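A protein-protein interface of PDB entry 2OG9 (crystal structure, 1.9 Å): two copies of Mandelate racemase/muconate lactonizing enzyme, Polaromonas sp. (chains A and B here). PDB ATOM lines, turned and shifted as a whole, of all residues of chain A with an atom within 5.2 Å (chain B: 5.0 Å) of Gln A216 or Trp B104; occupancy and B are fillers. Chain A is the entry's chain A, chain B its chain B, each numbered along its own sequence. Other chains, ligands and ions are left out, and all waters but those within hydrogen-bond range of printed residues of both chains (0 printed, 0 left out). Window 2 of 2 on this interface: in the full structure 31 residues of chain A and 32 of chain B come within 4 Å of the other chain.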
ATOM      1  N   ARG A  70      10.742  34.126   1.486  1.00  0.00           N
ATOM      2  CA  ARG A  70      12.148  34.485   1.652  1.00  0.00           C
ATOM      3  C   ARG A  70      12.635  34.997   0.293  1.00  0.00           C
ATOM      4  O   ARG A  70      11.823  35.429  -0.518  1.00  0.00           O
ATOM      5  CB  ARG A  70      12.981  33.292   2.147  1.00  0.00           C
ATOM      6  CG  ARG A  70      12.574  32.848   3.554  1.00  0.00           C
ATOM      7  CD  ARG A  70      13.476  31.763   4.125  1.00  0.00           C
ATOM      8  NE  ARG A  70      12.967  31.260   5.400  1.00  0.00           N
ATOM      9  CZ  ARG A  70      12.876  31.980   6.516  1.00  0.00           C
ATOM     10  NH1 ARG A  70      13.267  33.249   6.529  1.00  0.00           N
ATOM     11  NH2 ARG A  70      12.383  31.433   7.621  1.00  0.00           N
ATOM     12  N   ALA A 214       7.840  17.368   9.653  1.00  0.00           N
ATOM     13  CA  ALA A 214       9.179  17.470  10.238  1.00  0.00           C
ATOM     14  C   ALA A 214      10.046  18.525   9.565  1.00  0.00           C
ATOM     15  O   ALA A 214      11.150  18.818  10.027  1.00  0.00           O
ATOM     16  CB  ALA A 214       9.874  16.112  10.189  1.00  0.00           C
ATOM     17  N   ASN A 215       9.543  19.084   8.469  1.00  0.00           N
ATOM     18  CA  ASN A 215      10.243  20.119   7.714  1.00  0.00           C
ATOM     19  C   ASN A 215      11.722  19.840   7.434  1.00  0.00           C
ATOM     20  O   ASN A 215      12.585  20.670   7.736  1.00  0.00           O
ATOM     21  CB  ASN A 215      10.105  21.468   8.426  1.00  0.00           C
ATOM     22  CG  ASN A 215       8.656  21.855   8.663  1.00  0.00           C
ATOM     23  OD1 ASN A 215       7.960  21.229   9.468  1.00  0.00           O
ATOM     24  ND2 ASN A 215       8.190  22.882   7.955  1.00  0.00           N
ATOM     25  N   GLN A 216      12.006  18.677   6.851  1.00  0.00           N
ATOM     26  CA  GLN A 216      13.369  18.283   6.494  1.00  0.00           C
ATOM     27  C   GLN A 216      14.365  18.361   7.649  1.00  0.00           C
ATOM     28  O   GLN A 216      15.560  18.533   7.416  1.00  0.00           O
ATOM     29  CB  GLN A 216      13.896  19.168   5.355  1.00  0.00           C
ATOM     30  CG  GLN A 216      12.973  19.320   4.153  1.00  0.00           C
ATOM     31  CD  GLN A 216      13.588  20.168   3.048  1.00  0.00           C
ATOM     32  OE1 GLN A 216      14.594  19.794   2.449  1.00  0.00           O
ATOM     33  NE2 GLN A 216      12.983  21.319   2.778  1.00  0.00           N
ATOM     34  N   GLN A 217      13.898  18.221   8.884  1.00  0.00           N
ATOM     35  CA  GLN A 217      14.799  18.324  10.030  1.00  0.00           C
ATOM     36  C   GLN A 217      15.517  17.050  10.465  1.00  0.00           C
ATOM     37  O   GLN A 217      16.501  17.116  11.203  1.00  0.00           O
ATOM     38  CB  GLN A 217      14.049  18.898  11.236  1.00  0.00           C
ATOM     39  CG  GLN A 217      13.595  20.338  11.070  1.00  0.00           C
ATOM     40  CD  GLN A 217      14.705  21.243  10.575  1.00  0.00           C
ATOM     41  OE1 GLN A 217      14.904  21.401   9.367  1.00  0.00           O
ATOM     42  NE2 GLN A 217      15.448  21.832  11.507  1.00  0.00           N
ATOM     43  N   TRP A 218      15.043  15.894  10.018  1.00  0.00           N
ATOM     44  CA  TRP A 218      15.661  14.637  10.425  1.00  0.00           C
ATOM     45  C   TRP A 218      16.664  14.041   9.445  1.00  0.00           C
ATOM     46  O   TRP A 218      16.500  14.155   8.231  1.00  0.00           O
ATOM     47  CB  TRP A 218      14.588  13.580  10.678  1.00  0.00           C
ATOM     48  CG  TRP A 218      13.584  13.915  11.731  1.00  0.00           C
ATOM     49  CD1 TRP A 218      13.807  14.599  12.893  1.00  0.00           C
ATOM     50  CD2 TRP A 218      12.219  13.480  11.775  1.00  0.00           C
ATOM     51  NE1 TRP A 218      12.668  14.609  13.661  1.00  0.00           N
ATOM     52  CE2 TRP A 218      11.678  13.929  13.001  1.00  0.00           C
ATOM     53  CE3 TRP A 218      11.403  12.749  10.900  1.00  0.00           C
ATOM     54  CZ2 TRP A 218      10.353  13.669  13.376  1.00  0.00           C
ATOM     55  CZ3 TRP A 218      10.084  12.490  11.272  1.00  0.00           C
ATOM     56  CH2 TRP A 218       9.574  12.951  12.502  1.00  0.00           C
ATOM     57  N   GLU A 240       7.696  15.526   4.944  1.00  0.00           N
ATOM     58  CA  GLU A 240       9.084  15.963   4.834  1.00  0.00           C
ATOM     59  C   GLU A 240       9.998  15.486   5.958  1.00  0.00           C
ATOM     60  O   GLU A 240      10.666  16.291   6.606  1.00  0.00           O
ATOM     61  CB  GLU A 240       9.132  17.491   4.765  1.00  0.00           C
ATOM     62  CG  GLU A 240       8.689  18.079   3.440  1.00  0.00           C
ATOM     63  CD  GLU A 240       9.755  17.965   2.366  1.00  0.00           C
ATOM     64  OE1 GLU A 240       9.948  18.954   1.624  1.00  0.00           O
ATOM     65  OE2 GLU A 240      10.397  16.890   2.261  1.00  0.00           O
ATOM     66  N   PRO A 241      10.045  14.169   6.205  1.00  0.00           N
ATOM     67  CA  PRO A 241      10.917  13.687   7.279  1.00  0.00           C
ATOM     68  C   PRO A 241      12.398  13.915   6.981  1.00  0.00           C
ATOM     69  O   PRO A 241      13.203  14.068   7.898  1.00  0.00           O
ATOM     70  CB  PRO A 241      10.561  12.205   7.369  1.00  0.00           C
ATOM     71  CG  PRO A 241      10.195  11.866   5.933  1.00  0.00           C
ATOM     72  CD  PRO A 241       9.343  13.054   5.547  1.00  0.00           C
ATOM     73  N   LEU A 242      12.744  13.962   5.697  1.00  0.00           N
ATOM     74  CA  LEU A 242      14.134  14.144   5.270  1.00  0.00           C
ATOM     75  C   LEU A 242      14.305  15.306   4.299  1.00  0.00           C
ATOM     76  O   LEU A 242      13.338  15.971   3.939  1.00  0.00           O
ATOM     77  CB  LEU A 242      14.625  12.875   4.581  1.00  0.00           C
ATOM     78  CG  LEU A 242      14.571  11.578   5.389  1.00  0.00           C
ATOM     79  CD1 LEU A 242      14.807  10.393   4.461  1.00  0.00           C
ATOM     80  CD2 LEU A 242      15.610  11.625   6.501  1.00  0.00           C
ATOM     81  N   ASP A 243      15.546  15.537   3.873  1.00  0.00           N
ATOM     82  CA  ASP A 243      15.827  16.588   2.906  1.00  0.00           C
ATOM     83  C   ASP A 243      14.920  16.327   1.705  1.00  0.00           C
ATOM     84  O   ASP A 243      14.788  15.188   1.252  1.00  0.00           O
ATOM     85  CB  ASP A 243      17.285  16.540   2.449  1.00  0.00           C
ATOM     86  CG  ASP A 243      17.580  17.545   1.349  1.00  0.00           C
ATOM     87  OD1 ASP A 243      17.715  18.750   1.651  1.00  0.00           O
ATOM     88  OD2 ASP A 243      17.660  17.133   0.175  1.00  0.00           O
ATOM     89  N   ALA A 244      14.307  17.385   1.189  1.00  0.00           N
ATOM     90  CA  ALA A 244      13.396  17.282   0.055  1.00  0.00           C
ATOM     91  C   ALA A 244      13.970  16.518  -1.139  1.00  0.00           C
ATOM     92  O   ALA A 244      13.227  15.939  -1.932  1.00  0.00           O
ATOM     93  CB  ALA A 244      12.967  18.681  -0.383  1.00  0.00           C
ATOM     94  N   TYR A 245      15.292  16.505  -1.262  1.00  0.00           N
ATOM     95  CA  TYR A 245      15.926  15.831  -2.387  1.00  0.00           C
ATOM     96  C   TYR A 245      16.463  14.427  -2.126  1.00  0.00           C
ATOM     97  O   TYR A 245      17.028  13.806  -3.025  1.00  0.00           O
ATOM     98  CB  TYR A 245      17.027  16.733  -2.953  1.00  0.00           C
ATOM     99  CG  TYR A 245      16.453  17.941  -3.655  1.00  0.00           C
ATOM    100  CD1 TYR A 245      16.068  17.871  -4.990  1.00  0.00           C
ATOM    101  CD2 TYR A 245      16.197  19.123  -2.958  1.00  0.00           C
ATOM    102  CE1 TYR A 245      15.432  18.943  -5.616  1.00  0.00           C
ATOM    103  CE2 TYR A 245      15.561  20.202  -3.574  1.00  0.00           C
ATOM    104  CZ  TYR A 245      15.180  20.101  -4.900  1.00  0.00           C
ATOM    105  OH  TYR A 245      14.529  21.145  -5.513  1.00  0.00           O
ATOM    106  N   MET A 266       8.715  21.210  -1.703  1.00  0.00           N
ATOM    107  CA  MET A 266       9.880  22.041  -2.015  1.00  0.00           C
ATOM    108  C   MET A 266      10.325  22.012  -3.475  1.00  0.00           C
ATOM    109  O   MET A 266      11.082  22.883  -3.917  1.00  0.00           O
ATOM    110  CB  MET A 266      11.069  21.625  -1.143  1.00  0.00           C
ATOM    111  CG  MET A 266      10.824  21.754   0.348  1.00  0.00           C
ATOM    112  SD  MET A 266      10.336  23.562   0.822  1.00  0.00           S
ATOM    113  CE  MET A 266      12.037  24.416   0.446  1.00  0.00           C
ATOM    114  N   ASP B 100      25.322  26.728  -0.105  1.00  0.00           N
ATOM    115  CA  ASP B 100      24.129  26.174   0.540  1.00  0.00           C
ATOM    116  C   ASP B 100      23.344  27.228   1.319  1.00  0.00           C
ATOM    117  O   ASP B 100      22.117  27.226   1.297  1.00  0.00           O
ATOM    118  CB  ASP B 100      24.501  25.027   1.493  1.00  0.00           C
ATOM    119  CG  ASP B 100      24.955  23.772   0.763  1.00  0.00           C
ATOM    120  OD1 ASP B 100      24.730  23.663  -0.464  1.00  0.00           O
ATOM    121  OD2 ASP B 100      25.526  22.879   1.426  1.00  0.00           O
ATOM    122  N   LYS B 101      24.047  28.122   2.016  1.00  0.00           N
ATOM    123  CA  LYS B 101      23.370  29.163   2.782  1.00  0.00           C
ATOM    124  C   LYS B 101      22.593  30.104   1.864  1.00  0.00           C
ATOM    125  O   LYS B 101      21.460  30.480   2.165  1.00  0.00           O
ATOM    126  CB  LYS B 101      24.372  29.982   3.607  1.00  0.00           C
ATOM    127  CG  LYS B 101      23.705  31.079   4.437  1.00  0.00           C
ATOM    128  CD  LYS B 101      24.714  32.030   5.081  1.00  0.00           C
ATOM    129  CE  LYS B 101      24.002  33.136   5.864  1.00  0.00           C
ATOM    130  NZ  LYS B 101      24.944  34.116   6.487  1.00  0.00           N
ATOM    131  N   LEU B 102      23.197  30.492   0.747  1.00  0.00           N
ATOM    132  CA  LEU B 102      22.517  31.389  -0.179  1.00  0.00           C
ATOM    133  C   LEU B 102      21.342  30.682  -0.832  1.00  0.00           C
ATOM    134  O   LEU B 102      20.312  31.300  -1.121  1.00  0.00           O
ATOM    135  CB  LEU B 102      23.479  31.890  -1.256  1.00  0.00           C
ATOM    136  CG  LEU B 102      24.591  32.824  -0.778  1.00  0.00           C
ATOM    137  CD1 LEU B 102      25.278  33.434  -1.991  1.00  0.00           C
ATOM    138  CD2 LEU B 102      24.016  33.919   0.109  1.00  0.00           C
ATOM    139  N   CYS B 103      21.496  29.386  -1.067  1.00  0.00           N
ATOM    140  CA  CYS B 103      20.424  28.610  -1.675  1.00  0.00           C
ATOM    141  C   CYS B 103      19.258  28.543  -0.685  1.00  0.00           C
ATOM    142  O   CYS B 103      18.103  28.723  -1.066  1.00  0.00           O
ATOM    143  CB  CYS B 103      20.917  27.204  -2.012  1.00  0.00           C
ATOM    144  SG  CYS B 103      19.784  26.258  -3.057  1.00  0.00           S
ATOM    145  N   TRP B 104      19.562  28.300   0.588  1.00  0.00           N
ATOM    146  CA  TRP B 104      18.512  28.234   1.605  1.00  0.00           C
ATOM    147  C   TRP B 104      17.840  29.592   1.772  1.00  0.00           C
ATOM    148  O   TRP B 104      16.637  29.669   2.031  1.00  0.00           O
ATOM    149  CB  TRP B 104      19.075  27.776   2.957  1.00  0.00           C
ATOM    150  CG  TRP B 104      19.266  26.289   3.065  1.00  0.00           C
ATOM    151  CD1 TRP B 104      20.453  25.612   3.116  1.00  0.00           C
ATOM    152  CD2 TRP B 104      18.235  25.294   3.127  1.00  0.00           C
ATOM    153  NE1 TRP B 104      20.226  24.258   3.206  1.00  0.00           N
ATOM    154  CE2 TRP B 104      18.872  24.035   3.213  1.00  0.00           C
ATOM    155  CE3 TRP B 104      16.833  25.343   3.117  1.00  0.00           C
ATOM    156  CZ2 TRP B 104      18.155  22.832   3.288  1.00  0.00           C
ATOM    157  CZ3 TRP B 104      16.118  24.144   3.192  1.00  0.00           C
ATOM    158  CH2 TRP B 104      16.785  22.908   3.276  1.00  0.00           C
ATOM    159  N   ALA B 105      18.614  30.663   1.621  1.00  0.00           N
ATOM    160  CA  ALA B 105      18.071  32.010   1.753  1.00  0.00           C
ATOM    161  C   ALA B 105      16.959  32.235   0.731  1.00  0.00           C
ATOM    162  O   ALA B 105      16.120  33.119   0.910  1.00  0.00           O
ATOM    163  CB  ALA B 105      19.176  33.050   1.565  1.00  0.00           C
ATOM    164  N   GLY B 106      16.970  31.443  -0.340  1.00  0.00           N
ATOM    165  CA  GLY B 106      15.951  31.554  -1.371  1.00  0.00           C
ATOM    166  C   GLY B 106      15.430  30.168  -1.706  1.00  0.00           C
ATOM    167  O   GLY B 106      15.255  29.815  -2.875  1.00  0.00           O
ATOM    168  N   ALA B 107      15.169  29.388  -0.661  1.00  0.00           N
ATOM    169  CA  ALA B 107      14.702  28.011  -0.802  1.00  0.00           C
ATOM    170  C   ALA B 107      13.496  27.780  -1.711  1.00  0.00           C
ATOM    171  O   ALA B 107      13.451  26.780  -2.426  1.00  0.00           O
ATOM    172  CB  ALA B 107      14.421  27.418   0.582  1.00  0.00           C
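No position is printed for both chains.
Of the printed residues of chain B, Arg A70 touches Ala B105 (3.4 Å).
Of chain B, only Trp B104 (3.9 Å) comes within 4 Å of Gln A216.
Glu A240 touches none of the printed residues of chain B.
Printed residues of chain B within 4 Å of Met A266: Ala B107 (3.8 Å).
Of chain A, only Gln A216 comes within 4 Å of Trp B104.
Printed residues of chain A within 4 Å of Ala B105: Arg A70 (3.4 Å).
Of the printed residues of chain A, Ala B107 touches Met A266.
The nearest residue of chain A that does not touch Trp B104 is Arg A70 (4.3 Å).
Printed residues of chain B that touch a printed residue of chain A: Trp B104, Ala B105 and Ala B107.
Of the 13 printed residues of chain A, 3 touch a printed residue of chain B.
Printed residues of chain A that touch a printed residue of chain B: Arg A70, Gln A216 and Met A266.
Among the printed residues, 3 pairs touch across the chains.
Among the printed residues, pairs that only touch across the chains: Arg A70 with Ala B105, Gln A216 with Trp B104 and Met A266 with Ala B107.
The backbone carbonyl oxygen (O) of Glu A240 sits at hydrogen-bond distance from the backbone NH (N) of Gln A216, at 2.7 Å.
The side-chain carboxylate (OD1) of Asp A243 lies close to the side-chain amide oxygen (OE1) of Gln A216 (3.4 Å).
The backbone NH (N) of Ala A244 lies within hydrogen-bond range of the side-chain amide oxygen (OE1) of Gln A216 (2.7 Å).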
